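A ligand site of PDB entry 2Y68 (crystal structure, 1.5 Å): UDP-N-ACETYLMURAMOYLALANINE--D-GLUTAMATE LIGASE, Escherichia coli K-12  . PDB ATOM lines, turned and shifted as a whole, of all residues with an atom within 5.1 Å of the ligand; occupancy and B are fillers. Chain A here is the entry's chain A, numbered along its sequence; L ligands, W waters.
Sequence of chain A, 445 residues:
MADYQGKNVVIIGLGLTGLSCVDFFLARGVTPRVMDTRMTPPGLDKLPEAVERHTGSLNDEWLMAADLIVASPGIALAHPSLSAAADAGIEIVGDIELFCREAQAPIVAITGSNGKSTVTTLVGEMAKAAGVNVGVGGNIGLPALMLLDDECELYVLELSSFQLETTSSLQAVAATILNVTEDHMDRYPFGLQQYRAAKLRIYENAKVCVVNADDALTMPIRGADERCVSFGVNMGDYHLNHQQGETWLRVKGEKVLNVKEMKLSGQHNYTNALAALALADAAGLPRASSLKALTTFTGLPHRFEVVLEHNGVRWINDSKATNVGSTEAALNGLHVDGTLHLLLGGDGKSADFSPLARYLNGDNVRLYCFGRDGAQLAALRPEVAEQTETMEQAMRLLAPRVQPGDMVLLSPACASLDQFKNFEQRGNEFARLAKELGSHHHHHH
Water W7 lies within hydrogen-bond range of O4 of the ligand (2.6 Å), OG1 of Thr 322 (2.7 Å), OD2 of Asp 183 (2.7 Å) and NZ of Lys 349 (3.0 Å).
OG of Ser 72 sits at hydrogen-bond distance from N of Gly 74.
The backbone carbonyl oxygen of Thr 322 sits at hydrogen-bond distance from the side-chain amino group of Lys 349, at 2.8 Å.
The backbone NH (N) of Phe 162 sits close to the side-chain hydroxyl (OG) of Ser 160.
The backbone carbonyl oxygen (O) of Ile 12 sits at hydrogen-bond distance from the backbone NH (N) of Ser 72 (2.9 Å).
The backbone NH (N) of Gly 13 lies within hydrogen-bond range of the backbone carbonyl oxygen (O) of Met 35, 2.7 Å away.
OD2 of Asp 183 lies within hydrogen-bond range of NE2 of His 184, 3.4 Å away.
The guanidinium group (NH2) of Arg 38 is in salt-bridge range of the side-chain carboxylate (OD2) of Asp 36 (2.8 Å).
The side-chain amino group of Lys 349 lies within salt-bridge range of the side-chain carboxylate of Asp 183, at 2.8 Å.
Ile 12 touches the ligand (CG2 to S2, 3.5 Å).
Gly 13 touches the ligand (N to S2, 3.8 Å).
Asp 36 touches the ligand (OD1 to N3, 3.5 Å).
OG of Ser 72 touches C16 of the ligand, at 3.2 Å.
Gly 74 touches the ligand (CA to C17, 3.7 Å).
CD1 of Ile 75 touches S2 of the ligand (3.98 Å).
OD1 of Asn 139 touches C10 of the ligand, at 3.7 Å.
Ser 160 touches the ligand.
Phe 162 touches the ligand (CE2 to F1, 3.2 Å).
His 184 touches the ligand (CE1 to O4, 3.2 Å).
OG1 of Thr 322 touches O4 of the ligand (3.997 Å).
Ala 415 touches the ligand (CB to O3, 3.2 Å).
CD2 of Leu 417 touches C1 of the ligand (3.8 Å).
CA of Asn 422 touches O1 of the ligand, at 3.5 Å.
Hydrophobic or aromatic side chains within 4 Å of the ligand: Ile 12, Ile 75, Phe 162, His 184, Ala 415, Leu 417 and Phe 423.
The nearest printed residue that does not touch the ligand is Pro 73 (4.1 Å).
N3 of the ligand lies within hydrogen-bond range of OG1 of Thr 37 (2.7 Å).
The backbone NH (N) of Phe 423 is in hydrogen-bond range of an oxygen (O1) of the ligand (2.9 Å).
The side-chain hydroxyl (OG) of Ser 416 lies within hydrogen-bond range of an oxygen (O2) of the ligand (2.6 Å).
An oxygen (O3) of the ligand lies within salt-bridge range of the side-chain amino group of Lys 349 (2.8 Å).
The guanidinium group (NH2) of Arg 38 sits close to a sulfur (S1) of the ligand.
N of Ser 416 sits at hydrogen-bond distance from O2 of the ligand, at 2.7 Å.
The backbone NH (N) of Thr 37 sits close to a sulfur (S2) of the ligand (3.4 Å).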
ATOM      1  N   ILE A  12      16.253 -14.444  14.240  1.00  0.00           N
ATOM      2  CA  ILE A  12      17.548 -13.882  14.594  1.00  0.00           C
ATOM      3  C   ILE A  12      17.574 -13.639  16.079  1.00  0.00           C
ATOM      4  O   ILE A  12      16.758 -12.876  16.618  1.00  0.00           O
ATOM      5  CB  ILE A  12      17.826 -12.557  13.893  1.00  0.00           C
ATOM      6  CG1 ILE A  12      17.623 -12.667  12.385  1.00  0.00           C
ATOM      7  CG2 ILE A  12      19.229 -12.023  14.300  1.00  0.00           C
ATOM      8  CD1 ILE A  12      17.869 -11.339  11.695  1.00  0.00           C
ATOM      9  N   GLY A  13      18.460 -14.353  16.770  1.00  0.00           N
ATOM     10  CA  GLY A  13      18.562 -14.213  18.214  1.00  0.00           C
ATOM     11  C   GLY A  13      17.868 -15.355  18.935  1.00  0.00           C
ATOM     12  O   GLY A  13      16.665 -15.629  18.733  1.00  0.00           O
ATOM     13  N   MET A  35      19.554 -17.879  13.491  1.00  0.00           N
ATOM     14  CA  MET A  35      20.931 -17.345  13.508  1.00  0.00           C
ATOM     15  C   MET A  35      21.103 -16.425  14.700  1.00  0.00           C
ATOM     16  O   MET A  35      20.116 -15.866  15.235  1.00  0.00           O
ATOM     17  CB  MET A  35      21.280 -16.591  12.209  1.00  0.00           C
ATOM     18  CG  MET A  35      20.423 -15.396  11.957  1.00  0.00           C
ATOM     19  SD  MET A  35      20.813 -14.653  10.359  1.00  0.00           S
ATOM     20  CE  MET A  35      20.463 -16.006   9.259  1.00  0.00           C
ATOM     21  N   ASP A  36      22.347 -16.237  15.127  1.00  0.00           N
ATOM     22  CA  ASP A  36      22.641 -15.395  16.279  1.00  0.00           C
ATOM     23  C   ASP A  36      24.085 -14.939  16.137  1.00  0.00           C
ATOM     24  O   ASP A  36      24.930 -15.749  15.731  1.00  0.00           O
ATOM     25  CB  ASP A  36      22.474 -16.197  17.581  1.00  0.00           C
ATOM     26  CG  ASP A  36      22.431 -15.312  18.823  1.00  0.00           C
ATOM     27  OD1 ASP A  36      23.402 -14.543  19.073  1.00  0.00           O
ATOM     28  OD2 ASP A  36      21.394 -15.342  19.532  1.00  0.00           O
ATOM     29  N   THR A  37      24.373 -13.660  16.372  1.00  0.00           N
ATOM     30  CA  THR A  37      25.724 -13.160  16.173  1.00  0.00           C
ATOM     31  C   THR A  37      26.677 -13.691  17.250  1.00  0.00           C
ATOM     32  O   THR A  37      27.905 -13.619  17.087  1.00  0.00           O
ATOM     33  CB  THR A  37      25.825 -11.603  16.135  1.00  0.00           C
ATOM     34  OG1 THR A  37      25.420 -11.085  17.402  1.00  0.00           O
ATOM     35  CG2 THR A  37      24.957 -11.023  15.012  1.00  0.00           C
ATOM     36  N   ARG A  38      26.108 -14.209  18.329  1.00  0.00           N
ATOM     37  CA  ARG A  38      26.926 -14.814  19.410  1.00  0.00           C
ATOM     38  C   ARG A  38      27.337 -16.244  19.051  1.00  0.00           C
ATOM     39  O   ARG A  38      26.562 -16.989  18.486  1.00  0.00           O
ATOM     40  CB  ARG A  38      26.133 -14.751  20.722  1.00  0.00           C
ATOM     41  CG  ARG A  38      25.810 -13.313  21.136  1.00  0.00           C
ATOM     42  CD  ARG A  38      24.797 -13.255  22.255  1.00  0.00           C
ATOM     43  NE  ARG A  38      23.480 -13.704  21.813  1.00  0.00           N
ATOM     44  CZ  ARG A  38      22.386 -13.697  22.578  1.00  0.00           C
ATOM     45  NH1 ARG A  38      22.427 -13.245  23.827  1.00  0.00           N
ATOM     46  NH2 ARG A  38      21.247 -14.136  22.073  1.00  0.00           N
ATOM     47  N   LEU A  58      25.692 -13.093  11.372  1.00  0.00           N
ATOM     48  CA  LEU A  58      24.483 -13.293  10.596  1.00  0.00           C
ATOM     49  C   LEU A  58      24.846 -13.947   9.262  1.00  0.00           C
ATOM     50  O   LEU A  58      25.953 -13.788   8.745  1.00  0.00           O
ATOM     51  CB  LEU A  58      23.748 -11.967  10.369  1.00  0.00           C
ATOM     52  CG  LEU A  58      23.350 -11.274  11.686  1.00  0.00           C
ATOM     53  CD1 LEU A  58      22.520 -10.023  11.357  1.00  0.00           C
ATOM     54  CD2 LEU A  58      22.538 -12.216  12.601  1.00  0.00           C
ATOM     55  N   SER A  72      15.041 -10.609  17.101  1.00  0.00           N
ATOM     56  CA  SER A  72      15.114 -10.374  18.534  1.00  0.00           C
ATOM     57  C   SER A  72      15.220  -8.889  18.792  1.00  0.00           C
ATOM     58  O   SER A  72      15.802  -8.184  18.006  1.00  0.00           O
ATOM     59  CB  SER A  72      16.410 -11.020  19.044  1.00  0.00           C
ATOM     60  OG  SER A  72      16.684 -10.642  20.401  1.00  0.00           O
ATOM     61  N   PRO A  73      14.673  -8.416  19.911  1.00  0.00           N
ATOM     62  CA  PRO A  73      14.940  -7.032  20.308  1.00  0.00           C
ATOM     63  C   PRO A  73      16.421  -6.749  20.493  1.00  0.00           C
ATOM     64  O   PRO A  73      16.825  -5.590  20.453  1.00  0.00           O
ATOM     65  CB  PRO A  73      14.189  -6.886  21.640  1.00  0.00           C
ATOM     66  CG  PRO A  73      13.977  -8.266  22.145  1.00  0.00           C
ATOM     67  CD  PRO A  73      13.796  -9.108  20.884  1.00  0.00           C
ATOM     68  N   GLY A  74      17.236  -7.813  20.623  1.00  0.00           N
ATOM     69  CA  GLY A  74      18.669  -7.650  20.819  1.00  0.00           C
ATOM     70  C   GLY A  74      19.490  -7.423  19.570  1.00  0.00           C
ATOM     71  O   GLY A  74      20.713  -7.185  19.677  1.00  0.00           O
ATOM     72  N   ILE A  75      18.852  -7.446  18.394  1.00  0.00           N
ATOM     73  CA  ILE A  75      19.582  -7.145  17.172  1.00  0.00           C
ATOM     74  C   ILE A  75      19.056  -5.854  16.592  1.00  0.00           C
ATOM     75  O   ILE A  75      17.844  -5.688  16.409  1.00  0.00           O
ATOM     76  CB  ILE A  75      19.532  -8.316  16.127  1.00  0.00           C
ATOM     77  CG1 ILE A  75      20.495  -8.034  14.970  1.00  0.00           C
ATOM     78  CG2 ILE A  75      18.121  -8.545  15.605  1.00  0.00           C
ATOM     79  CD1 ILE A  75      21.922  -8.360  15.335  1.00  0.00           C
ATOM     80  N   ASN A 139       8.605  -8.450  28.251  1.00  0.00           N
ATOM     81  CA  ASN A 139      10.002  -8.102  28.415  1.00  0.00           C
ATOM     82  C   ASN A 139      10.517  -8.556  29.784  1.00  0.00           C
ATOM     83  O   ASN A 139      11.722  -8.612  29.993  1.00  0.00           O
ATOM     84  CB  ASN A 139      10.194  -6.583  28.176  1.00  0.00           C
ATOM     85  CG  ASN A 139      11.652  -6.181  28.108  1.00  0.00           C
ATOM     86  OD1 ASN A 139      12.437  -6.772  27.375  1.00  0.00           O
ATOM     87  ND2 ASN A 139      12.008  -5.142  28.850  1.00  0.00           N
ATOM     88  N   SER A 160       9.609  -3.444  25.531  1.00  0.00           N
ATOM     89  CA  SER A 160      10.771  -2.549  25.401  1.00  0.00           C
ATOM     90  C   SER A 160      10.637  -1.702  24.145  1.00  0.00           C
ATOM     91  O   SER A 160       9.882  -2.022  23.200  1.00  0.00           O
ATOM     92  CB  SER A 160      12.076  -3.342  25.287  1.00  0.00           C
ATOM     93  OG  SER A 160      12.070  -4.170  24.126  1.00  0.00           O
ATOM     94  N   PHE A 162      12.736  -1.613  21.864  1.00  0.00           N
ATOM     95  CA  PHE A 162      13.227  -2.462  20.776  1.00  0.00           C
ATOM     96  C   PHE A 162      12.114  -3.382  20.291  1.00  0.00           C
ATOM     97  O   PHE A 162      11.936  -3.526  19.079  1.00  0.00           O
ATOM     98  CB  PHE A 162      14.417  -3.298  21.254  1.00  0.00           C
ATOM     99  CG  PHE A 162      15.586  -2.476  21.800  1.00  0.00           C
ATOM    100  CD1 PHE A 162      15.994  -1.318  21.173  1.00  0.00           C
ATOM    101  CD2 PHE A 162      16.279  -2.919  22.921  1.00  0.00           C
ATOM    102  CE1 PHE A 162      17.083  -0.562  21.678  1.00  0.00           C
ATOM    103  CE2 PHE A 162      17.363  -2.191  23.401  1.00  0.00           C
ATOM    104  CZ  PHE A 162      17.749  -1.028  22.784  1.00  0.00           C
ATOM    105  N   ASP A 183      18.257   6.653  27.480  1.00  0.00           N
ATOM    106  CA  ASP A 183      18.702   5.288  27.649  1.00  0.00           C
ATOM    107  C   ASP A 183      18.968   4.701  26.273  1.00  0.00           C
ATOM    108  O   ASP A 183      18.471   5.241  25.263  1.00  0.00           O
ATOM    109  CB  ASP A 183      17.645   4.486  28.431  1.00  0.00           C
ATOM    110  CG  ASP A 183      18.213   3.170  29.035  1.00  0.00           C
ATOM    111  OD1 ASP A 183      19.421   2.845  28.896  1.00  0.00           O
ATOM    112  OD2 ASP A 183      17.354   2.455  29.590  1.00  0.00           O
ATOM    113  N   HIS A 184      19.717   3.606  26.218  1.00  0.00           N
ATOM    114  CA  HIS A 184      19.900   2.821  24.986  1.00  0.00           C
ATOM    115  C   HIS A 184      20.472   3.672  23.857  1.00  0.00           C
ATOM    116  O   HIS A 184      20.210   3.376  22.706  1.00  0.00           O
ATOM    117  CB  HIS A 184      18.547   2.217  24.572  1.00  0.00           C
ATOM    118  CG  HIS A 184      17.975   1.289  25.595  1.00  0.00           C
ATOM    119  ND1 HIS A 184      18.643   0.169  26.024  1.00  0.00           N
ATOM    120  CD2 HIS A 184      16.815   1.343  26.280  1.00  0.00           C
ATOM    121  CE1 HIS A 184      17.904  -0.451  26.931  1.00  0.00           C
ATOM    122  NE2 HIS A 184      16.785   0.231  27.104  1.00  0.00           N
ATOM    123  N   THR A 322      19.387   0.555  35.653  1.00  0.00           N
ATOM    124  CA  THR A 322      20.315   0.366  34.549  1.00  0.00           C
ATOM    125  C   THR A 322      20.427   1.612  33.679  1.00  0.00           C
ATOM    126  O   THR A 322      21.059   1.603  32.650  1.00  0.00           O
ATOM    127  CB  THR A 322      19.866  -0.836  33.686  1.00  0.00           C
ATOM    128  OG1 THR A 322      18.476  -0.636  33.328  1.00  0.00           O
ATOM    129  CG2 THR A 322      20.012  -2.135  34.483  1.00  0.00           C
ATOM    130  N   LYS A 349      26.162   2.750  28.263  1.00  0.00           N
ATOM    131  CA  LYS A 349      25.471   2.897  26.966  1.00  0.00           C
ATOM    132  C   LYS A 349      25.563   4.301  26.400  1.00  0.00           C
ATOM    133  O   LYS A 349      24.603   4.794  25.786  1.00  0.00           O
ATOM    134  CB  LYS A 349      24.002   2.480  27.080  1.00  0.00           C
ATOM    135  CG  LYS A 349      23.815   0.994  27.362  1.00  0.00           C
ATOM    136  CD  LYS A 349      22.406   0.691  27.899  1.00  0.00           C
ATOM    137  CE  LYS A 349      22.358   0.953  29.434  1.00  0.00           C
ATOM    138  NZ  LYS A 349      20.978   0.791  29.935  1.00  0.00           N
ATOM    139  N   CYS A 414      23.700   1.827  35.014  1.00  0.00           N
ATOM    140  CA  CYS A 414      24.347   1.230  33.826  1.00  0.00           C
ATOM    141  C   CYS A 414      23.845  -0.190  33.646  1.00  0.00           C
ATOM    142  O   CYS A 414      23.444  -0.833  34.602  1.00  0.00           O
ATOM    143  CB  CYS A 414      25.879   1.124  34.019  1.00  0.00           C
ATOM    144  SG  CYS A 414      26.737   2.653  34.279  1.00  0.00           S
ATOM    145  N   ALA A 415      23.958  -0.695  32.422  1.00  0.00           N
ATOM    146  CA  ALA A 415      23.793  -2.135  32.209  1.00  0.00           C
ATOM    147  C   ALA A 415      24.926  -2.916  32.872  1.00  0.00           C
ATOM    148  O   ALA A 415      26.027  -2.389  33.101  1.00  0.00           O
ATOM    149  CB  ALA A 415      23.705  -2.451  30.724  1.00  0.00           C
ATOM    150  N   SER A 416      24.602  -4.151  33.225  1.00  0.00           N
ATOM    151  CA  SER A 416      25.538  -5.049  33.886  1.00  0.00           C
ATOM    152  C   SER A 416      26.327  -5.910  32.898  1.00  0.00           C
ATOM    153  O   SER A 416      27.204  -6.662  33.331  1.00  0.00           O
ATOM    154  CB  SER A 416      24.780  -5.989  34.829  1.00  0.00           C
ATOM    155  OG  SER A 416      24.044  -6.944  34.086  1.00  0.00           O
ATOM    156  N   LEU A 417      26.025  -5.796  31.620  1.00  0.00           N
ATOM    157  CA  LEU A 417      26.369  -6.848  30.649  1.00  0.00           C
ATOM    158  C   LEU A 417      27.851  -6.969  30.314  1.00  0.00           C
ATOM    159  O   LEU A 417      28.296  -7.986  29.741  1.00  0.00           O
ATOM    160  CB  LEU A 417      25.525  -6.667  29.383  1.00  0.00           C
ATOM    161  CG  LEU A 417      23.999  -6.659  29.604  1.00  0.00           C
ATOM    162  CD1 LEU A 417      23.237  -6.529  28.284  1.00  0.00           C
ATOM    163  CD2 LEU A 417      23.538  -7.898  30.377  1.00  0.00           C
ATOM    164  N   ASN A 422      23.364 -10.523  33.608  1.00  0.00           N
ATOM    165  CA  ASN A 422      22.170  -9.666  33.660  1.00  0.00           C
ATOM    166  C   ASN A 422      22.112  -8.978  35.002  1.00  0.00           C
ATOM    167  O   ASN A 422      22.910  -9.296  35.911  1.00  0.00           O
ATOM    168  CB  ASN A 422      20.859 -10.431  33.385  1.00  0.00           C
ATOM    169  CG  ASN A 422      20.698 -11.697  34.232  1.00  0.00           C
ATOM    170  OD1 ASN A 422      21.061 -11.737  35.416  1.00  0.00           O
ATOM    171  ND2 ASN A 422      20.127 -12.731  33.623  1.00  0.00           N
ATOM    172  N   PHE A 423      21.178  -8.038  35.154  1.00  0.00           N
ATOM    173  CA  PHE A 423      21.161  -7.214  36.379  1.00  0.00           C
ATOM    174  C   PHE A 423      20.741  -8.056  37.570  1.00  0.00           C
ATOM    175  O   PHE A 423      21.105  -7.723  38.696  1.00  0.00           O
ATOM    176  CB  PHE A 423      20.243  -5.983  36.225  1.00  0.00           C
ATOM    177  CG  PHE A 423      18.792  -6.339  36.199  1.00  0.00           C
ATOM    178  CD1 PHE A 423      18.074  -6.517  37.380  1.00  0.00           C
ATOM    179  CD2 PHE A 423      18.170  -6.582  34.982  1.00  0.00           C
ATOM    180  CE1 PHE A 423      16.729  -6.914  37.359  1.00  0.00           C
ATOM    181  CE2 PHE A 423      16.815  -6.959  34.915  1.00  0.00           C
ATOM    182  CZ  PHE A 423      16.098  -7.130  36.125  1.00  0.00           C
ATOM    183  N   GLU A 424      20.038  -9.166  37.336  1.00  0.00           N
ATOM    184  CA  GLU A 424      19.673 -10.051  38.451  1.00  0.00           C
ATOM    185  C   GLU A 424      20.922 -10.683  39.043  1.00  0.00           C
ATOM    186  O   GLU A 424      21.059 -10.798  40.257  1.00  0.00           O
ATOM    187  CB  GLU A 424      18.755 -11.178  37.965  1.00  0.00           C
ATOM    188  CG  GLU A 424      17.379 -10.697  37.694  1.00  0.00           C
ATOM    189  CD  GLU A 424      17.154 -10.419  36.229  1.00  0.00           C
ATOM    190  OE1 GLU A 424      18.134 -10.167  35.490  1.00  0.00           O
ATOM    191  OE2 GLU A 424      15.990 -10.485  35.800  1.00  0.00           O
ATOM    192  N   ARG A 426      23.908  -9.528  38.942  1.00  0.00           N
ATOM    193  CA  ARG A 426      24.592  -8.450  39.637  1.00  0.00           C
ATOM    194  C   ARG A 426      23.968  -8.179  41.015  1.00  0.00           C
ATOM    195  O   ARG A 426      24.669  -8.043  42.028  1.00  0.00           O
ATOM    196  CB  ARG A 426      24.613  -7.179  38.766  1.00  0.00           C
ATOM    197  CG  ARG A 426      25.116  -5.943  39.464  1.00  0.00           C
ATOM    198  CD  ARG A 426      25.245  -4.776  38.458  1.00  0.00           C
ATOM    199  NE  ARG A 426      23.937  -4.261  38.052  1.00  0.00           N
ATOM    200  CZ  ARG A 426      23.771  -3.356  37.103  1.00  0.00           C
ATOM    201  NH1 ARG A 426      24.827  -2.856  36.456  1.00  0.00           N
ATOM    202  NH2 ARG A 426      22.525  -2.933  36.819  1.00  0.00           N
HETATM  203  O1  LIG L   1      20.541  -6.747  32.614  1.00  0.00           O
HETATM  204  C1  LIG L   1      21.223  -5.685  32.469  1.00  0.00           C
HETATM  205  O2  LIG L   1      22.166  -5.318  33.167  1.00  0.00           O
HETATM  206  C2  LIG L   1      20.965  -4.804  31.304  1.00  0.00           C
HETATM  207  C3  LIG L   1      19.814  -4.916  30.700  1.00  0.00           C
HETATM  208  C4  LIG L   1      19.635  -2.637  29.537  1.00  0.00           C
HETATM  209  O3  LIG L   1      20.721  -1.975  29.528  1.00  0.00           O
HETATM  210  O4  LIG L   1      18.525  -2.103  29.610  1.00  0.00           O
HETATM  211  N1  LIG L   1      19.067  -4.754  28.538  1.00  0.00           N
HETATM  212  C5  LIG L   1      18.708  -4.297  27.346  1.00  0.00           C
HETATM  213  O5  LIG L   1      19.263  -3.365  26.796  1.00  0.00           O
HETATM  214  C6  LIG L   1      17.617  -5.107  26.700  1.00  0.00           C
HETATM  215  C7  LIG L   1      17.807  -6.493  26.702  1.00  0.00           C
HETATM  216  C8  LIG L   1      16.433  -4.571  26.159  1.00  0.00           C
HETATM  217  C9  LIG L   1      15.478  -5.411  25.616  1.00  0.00           C
HETATM  218  C10 LIG L   1      15.675  -6.790  25.596  1.00  0.00           C
HETATM  219  C11 LIG L   1      16.836  -7.322  26.137  1.00  0.00           C
HETATM  220  C12 LIG L   1      16.980  -8.795  26.152  1.00  0.00           C
HETATM  221  N2  LIG L   1      16.939  -9.486  24.940  1.00  0.00           N
HETATM  222  C13 LIG L   1      18.136  -9.693  24.290  1.00  0.00           C
HETATM  223  C14 LIG L   1      19.266  -8.957  24.643  1.00  0.00           C
HETATM  224  C15 LIG L   1      20.461  -9.171  23.963  1.00  0.00           C
HETATM  225  C16 LIG L   1      18.177 -10.626  23.265  1.00  0.00           C
HETATM  226  C17 LIG L   1      19.366 -10.852  22.589  1.00  0.00           C
HETATM  227  C18 LIG L   1      20.505 -10.143  22.958  1.00  0.00           C
HETATM  228  C19 LIG L   1      21.788 -10.242  22.236  1.00  0.00           C
HETATM  229  C20 LIG L   1      21.963 -10.639  20.829  1.00  0.00           C
HETATM  230  S1  LIG L   1      20.680 -11.171  19.777  1.00  0.00           S
HETATM  231  C21 LIG L   1      21.884 -11.356  18.544  1.00  0.00           C
HETATM  232  S2  LIG L   1      21.460 -11.958  16.970  1.00  0.00           S
HETATM  233  N3  LIG L   1      23.162 -11.048  18.837  1.00  0.00           N
HETATM  234  C22 LIG L   1      23.172 -10.647  20.141  1.00  0.00           C
HETATM  235  F1  LIG L   1      16.170  -3.232  26.141  1.00  0.00           F
HETATM  236  O6  LIG L   1      24.291 -10.270  20.683  1.00  0.00           O
HETATM  237  C23 LIG L   1      19.549  -4.096  29.509  1.00  0.00           C
HETATM  238  O   HOH W   1      22.720  -2.847  27.163  1.00  0.00           O
HETATM  239  O   HOH W   2      14.188  -1.332  27.374  1.00  0.00           O
HETATM  240  O   HOH W   3      14.110  -3.415  28.864  1.00  0.00           O
HETATM  241  O   HOH W   4      14.831  -6.976  28.845  1.00  0.00           O
HETATM  242  O   HOH W   5      14.483 -11.049  24.287  1.00  0.00           O
HETATM  243  O   HOH W   6      14.586  -1.062  24.798  1.00  0.00           O
HETATM  244  O   HOH W   7      18.153   0.156  30.798  1.00  0.00           O
HETATM  245  O   HOH W   8      20.853  -3.337  24.576  1.00  0.00           O
